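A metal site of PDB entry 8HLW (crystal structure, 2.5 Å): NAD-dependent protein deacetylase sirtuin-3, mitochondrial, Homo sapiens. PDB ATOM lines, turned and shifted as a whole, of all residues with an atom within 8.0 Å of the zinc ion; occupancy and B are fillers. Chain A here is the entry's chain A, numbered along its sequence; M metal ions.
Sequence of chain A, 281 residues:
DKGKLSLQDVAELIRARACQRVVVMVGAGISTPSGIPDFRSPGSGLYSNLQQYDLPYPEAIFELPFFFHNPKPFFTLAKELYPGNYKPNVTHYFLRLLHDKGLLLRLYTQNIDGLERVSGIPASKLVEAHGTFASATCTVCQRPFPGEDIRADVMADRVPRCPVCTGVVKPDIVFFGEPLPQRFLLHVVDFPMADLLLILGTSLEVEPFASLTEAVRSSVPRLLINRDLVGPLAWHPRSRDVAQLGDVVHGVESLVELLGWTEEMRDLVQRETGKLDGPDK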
ATOM      1  N   THR A 137      27.901  20.134 -34.630  1.00  0.00           N
ATOM      2  CA  THR A 137      26.535  19.713 -34.354  1.00  0.00           C
ATOM      3  C   THR A 137      26.544  18.284 -33.839  1.00  0.00           C
ATOM      4  O   THR A 137      27.222  17.419 -34.401  1.00  0.00           O
ATOM      5  CB  THR A 137      25.663  19.800 -35.604  1.00  0.00           C
ATOM      6  OG1 THR A 137      25.710  21.131 -36.134  1.00  0.00           O
ATOM      7  CG2 THR A 137      24.222  19.449 -35.276  1.00  0.00           C
ATOM      8  N   CYS A 138      25.794  18.045 -32.769  1.00  0.00           N
ATOM      9  CA  CYS A 138      25.663  16.703 -32.225  1.00  0.00           C
ATOM     10  C   CYS A 138      24.891  15.818 -33.200  1.00  0.00           C
ATOM     11  O   CYS A 138      23.859  16.219 -33.733  1.00  0.00           O
ATOM     12  CB  CYS A 138      24.949  16.752 -30.870  1.00  0.00           C
ATOM     13  SG  CYS A 138      24.619  15.150 -30.137  1.00  0.00           S
ATOM     14  N   THR A 139      25.404  14.610 -33.417  1.00  0.00           N
ATOM     15  CA  THR A 139      24.785  13.688 -34.373  1.00  0.00           C
ATOM     16  C   THR A 139      23.505  13.067 -33.842  1.00  0.00           C
ATOM     17  O   THR A 139      22.750  12.478 -34.632  1.00  0.00           O
ATOM     18  CB  THR A 139      25.781  12.584 -34.741  1.00  0.00           C
ATOM     19  OG1 THR A 139      26.159  11.873 -33.561  1.00  0.00           O
ATOM     20  CG2 THR A 139      27.018  13.171 -35.404  1.00  0.00           C
ATOM     21  N   VAL A 140      23.220  13.179 -32.551  1.00  0.00           N
ATOM     22  CA  VAL A 140      22.056  12.531 -31.951  1.00  0.00           C
ATOM     23  C   VAL A 140      20.940  13.550 -31.753  1.00  0.00           C
ATOM     24  O   VAL A 140      19.884  13.456 -32.374  1.00  0.00           O
ATOM     25  CB  VAL A 140      22.418  11.872 -30.606  1.00  0.00           C
ATOM     26  CG1 VAL A 140      21.231  11.070 -30.082  1.00  0.00           C
ATOM     27  CG2 VAL A 140      23.635  10.978 -30.755  1.00  0.00           C
ATOM     28  N   CYS A 141      21.169  14.524 -30.873  1.00  0.00           N
ATOM     29  CA  CYS A 141      20.155  15.501 -30.505  1.00  0.00           C
ATOM     30  C   CYS A 141      20.249  16.793 -31.306  1.00  0.00           C
ATOM     31  O   CYS A 141      19.451  17.698 -31.069  1.00  0.00           O
ATOM     32  CB  CYS A 141      20.257  15.802 -29.004  1.00  0.00           C
ATOM     33  SG  CYS A 141      21.649  16.858 -28.544  1.00  0.00           S
ATOM     34  N   GLN A 142      21.190  16.885 -32.232  1.00  0.00           N
ATOM     35  CA  GLN A 142      21.319  18.014 -33.154  1.00  0.00           C
ATOM     36  C   GLN A 142      21.678  19.324 -32.472  1.00  0.00           C
ATOM     37  O   GLN A 142      21.643  20.379 -33.113  1.00  0.00           O
ATOM     38  CB  GLN A 142      20.035  18.212 -33.969  1.00  0.00           C
ATOM     39  CG  GLN A 142      19.464  16.933 -34.562  1.00  0.00           C
ATOM     40  CD  GLN A 142      20.524  16.083 -35.248  1.00  0.00           C
ATOM     41  OE1 GLN A 142      20.615  14.878 -35.015  1.00  0.00           O
ATOM     42  NE2 GLN A 142      21.337  16.712 -36.083  1.00  0.00           N
ATOM     43  N   ARG A 143      22.022  19.287 -31.186  1.00  0.00           N
ATOM     44  CA  ARG A 143      22.393  20.513 -30.493  1.00  0.00           C
ATOM     45  C   ARG A 143      23.554  21.197 -31.220  1.00  0.00           C
ATOM     46  O   ARG A 143      24.542  20.527 -31.544  1.00  0.00           O
ATOM     47  CB  ARG A 143      22.800  20.197 -29.058  1.00  0.00           C
ATOM     48  CG  ARG A 143      22.445  21.275 -28.044  1.00  0.00           C
ATOM     49  CD  ARG A 143      22.830  20.837 -26.642  1.00  0.00           C
ATOM     50  NE  ARG A 143      21.964  21.432 -25.625  1.00  0.00           N
ATOM     51  CZ  ARG A 143      20.693  21.101 -25.429  1.00  0.00           C
ATOM     52  NH1 ARG A 143      20.098  20.180 -26.177  1.00  0.00           N
ATOM     53  NH2 ARG A 143      20.012  21.703 -24.456  1.00  0.00           N
ATOM     54  N   PRO A 144      23.482  22.489 -31.486  1.00  0.00           N
ATOM     55  CA  PRO A 144      24.621  23.194 -32.083  1.00  0.00           C
ATOM     56  C   PRO A 144      25.697  23.471 -31.047  1.00  0.00           C
ATOM     57  O   PRO A 144      25.451  23.511 -29.841  1.00  0.00           O
ATOM     58  CB  PRO A 144      24.005  24.491 -32.605  1.00  0.00           C
ATOM     59  CG  PRO A 144      22.870  24.755 -31.668  1.00  0.00           C
ATOM     60  CD  PRO A 144      22.336  23.402 -31.259  1.00  0.00           C
ATOM     61  N   PHE A 145      26.919  23.679 -31.548  1.00  0.00           N
ATOM     62  CA  PHE A 145      28.051  23.984 -30.683  1.00  0.00           C
ATOM     63  C   PHE A 145      29.036  24.852 -31.453  1.00  0.00           C
ATOM     64  O   PHE A 145      29.263  24.617 -32.640  1.00  0.00           O
ATOM     65  CB  PHE A 145      28.771  22.718 -30.199  1.00  0.00           C
ATOM     66  CG  PHE A 145      27.915  21.820 -29.355  1.00  0.00           C
ATOM     67  CD1 PHE A 145      27.735  22.072 -28.015  1.00  0.00           C
ATOM     68  CD2 PHE A 145      27.301  20.709 -29.916  1.00  0.00           C
ATOM     69  CE1 PHE A 145      26.957  21.244 -27.238  1.00  0.00           C
ATOM     70  CE2 PHE A 145      26.523  19.867 -29.150  1.00  0.00           C
ATOM     71  CZ  PHE A 145      26.354  20.137 -27.804  1.00  0.00           C
ATOM     72  N   ARG A 161      32.146  14.724 -27.635  1.00  0.00           N
ATOM     73  CA  ARG A 161      30.892  14.123 -27.211  1.00  0.00           C
ATOM     74  C   ARG A 161      29.974  15.178 -26.629  1.00  0.00           C
ATOM     75  O   ARG A 161      30.405  16.090 -25.926  1.00  0.00           O
ATOM     76  CB  ARG A 161      31.138  13.007 -26.185  1.00  0.00           C
ATOM     77  CG  ARG A 161      31.801  11.777 -26.784  1.00  0.00           C
ATOM     78  CD  ARG A 161      31.265  10.486 -26.206  1.00  0.00           C
ATOM     79  NE  ARG A 161      31.624   9.354 -27.062  1.00  0.00           N
ATOM     80  CZ  ARG A 161      30.818   8.780 -27.943  1.00  0.00           C
ATOM     81  NH1 ARG A 161      29.559   9.160 -28.079  1.00  0.00           N
ATOM     82  NH2 ARG A 161      31.285   7.796 -28.706  1.00  0.00           N
ATOM     83  N   CYS A 162      28.689  15.037 -26.939  1.00  0.00           N
ATOM     84  CA  CYS A 162      27.691  16.019 -26.523  1.00  0.00           C
ATOM     85  C   CYS A 162      27.595  16.056 -25.002  1.00  0.00           C
ATOM     86  O   CYS A 162      27.398  15.018 -24.365  1.00  0.00           O
ATOM     87  CB  CYS A 162      26.335  15.649 -27.128  1.00  0.00           C
ATOM     88  SG  CYS A 162      25.013  16.834 -26.824  1.00  0.00           S
ATOM     89  N   PRO A 163      27.721  17.235 -24.372  1.00  0.00           N
ATOM     90  CA  PRO A 163      27.549  17.311 -22.918  1.00  0.00           C
ATOM     91  C   PRO A 163      26.119  17.081 -22.456  1.00  0.00           C
ATOM     92  O   PRO A 163      25.857  17.125 -21.244  1.00  0.00           O
ATOM     93  CB  PRO A 163      27.997  18.747 -22.571  1.00  0.00           C
ATOM     94  CG  PRO A 163      28.724  19.254 -23.777  1.00  0.00           C
ATOM     95  CD  PRO A 163      28.112  18.536 -24.946  1.00  0.00           C
ATOM     96  N   VAL A 164      25.185  16.824 -23.369  1.00  0.00           N
ATOM     97  CA  VAL A 164      23.767  16.673 -23.048  1.00  0.00           C
ATOM     98  C   VAL A 164      23.317  15.222 -23.184  1.00  0.00           C
ATOM     99  O   VAL A 164      22.638  14.689 -22.311  1.00  0.00           O
ATOM    100  CB  VAL A 164      22.902  17.606 -23.919  1.00  0.00           C
ATOM    101  CG1 VAL A 164      21.463  17.109 -23.997  1.00  0.00           C
ATOM    102  CG2 VAL A 164      22.979  19.041 -23.402  1.00  0.00           C
ATOM    103  N   CYS A 165      23.680  14.577 -24.298  1.00  0.00           N
ATOM    104  CA  CYS A 165      23.286  13.199 -24.550  1.00  0.00           C
ATOM    105  C   CYS A 165      24.446  12.265 -24.815  1.00  0.00           C
ATOM    106  O   CYS A 165      24.224  11.076 -25.088  1.00  0.00           O
ATOM    107  CB  CYS A 165      22.312  13.142 -25.744  1.00  0.00           C
ATOM    108  SG  CYS A 165      23.094  13.418 -27.351  1.00  0.00           S
ATOM    109  N   THR A 166      25.684  12.749 -24.742  1.00  0.00           N
ATOM    110  CA  THR A 166      26.902  11.955 -24.930  1.00  0.00           C
ATOM    111  C   THR A 166      27.055  11.441 -26.352  1.00  0.00           C
ATOM    112  O   THR A 166      27.884  10.552 -26.599  1.00  0.00           O
ATOM    113  CB  THR A 166      26.942  10.768 -23.964  1.00  0.00           C
ATOM    114  OG1 THR A 166      26.347  11.138 -22.716  1.00  0.00           O
ATOM    115  CG2 THR A 166      28.386  10.326 -23.716  1.00  0.00           C
ATOM    116  N   GLY A 167      26.283  11.961 -27.301  1.00  0.00           N
ATOM    117  CA  GLY A 167      26.461  11.584 -28.689  1.00  0.00           C
ATOM    118  C   GLY A 167      27.720  12.209 -29.269  1.00  0.00           C
ATOM    119  O   GLY A 167      28.323  13.118 -28.698  1.00  0.00           O
ATOM    120  N   VAL A 168      28.112  11.700 -30.432  1.00  0.00           N
ATOM    121  CA  VAL A 168      29.278  12.232 -31.109  1.00  0.00           C
ATOM    122  C   VAL A 168      28.933  13.594 -31.707  1.00  0.00           C
ATOM    123  O   VAL A 168      27.920  13.746 -32.401  1.00  0.00           O
ATOM    124  CB  VAL A 168      29.773  11.270 -32.200  1.00  0.00           C
ATOM    125  CG1 VAL A 168      30.737  11.980 -33.150  1.00  0.00           C
ATOM    126  CG2 VAL A 168      30.445  10.071 -31.560  1.00  0.00           C
ATOM    127  N   VAL A 169      29.762  14.586 -31.427  1.00  0.00           N
ATOM    128  CA  VAL A 169      29.627  15.906 -32.019  1.00  0.00           C
ATOM    129  C   VAL A 169      30.499  15.955 -33.266  1.00  0.00           C
ATOM    130  O   VAL A 169      31.698  15.655 -33.211  1.00  0.00           O
ATOM    131  CB  VAL A 169      30.015  17.015 -31.028  1.00  0.00           C
ATOM    132  CG1 VAL A 169      29.901  18.373 -31.675  1.00  0.00           C
ATOM    133  CG2 VAL A 169      29.127  16.943 -29.799  1.00  0.00           C
HETATM  134 ZN    ZN M   1      23.547  15.565 -28.119  1.00  0.00          ZN
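The backbone NH (N) of Val 140 lies close to the side-chain sulfur (SG) of Cys 138, 3.4 Å away. The backbone NH of Cys 138 sits at hydrogen-bond distance from the backbone carbonyl oxygen of Arg 143 (3.0 Å). NE2 of Gln 142 sits close to O of Cys 138 (3.5 Å). N of Gly 167 sits close to SG of Cys 165 (3.5 Å). The backbone NH (N) of Cys 162 sits at hydrogen-bond distance from the backbone carbonyl oxygen (O) of Gly 167 (2.6 Å). The side-chain sulfur (SG) of Cys 162 lies close to the backbone NH (N) of Val 164 (3.5 Å). The side-chain sulfur (SG) of Cys 141 sits close to the backbone NH (N) of Arg 143 (3.6 Å).
Four residues have an atom within 4 Å of the zinc ion: Cys 138, Cys 141, Cys 162 and Cys 165.
The zinc ion is bound by SG of Cys 138, SG of Cys 165, SG of Cys 162 and SG of Cys 141.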
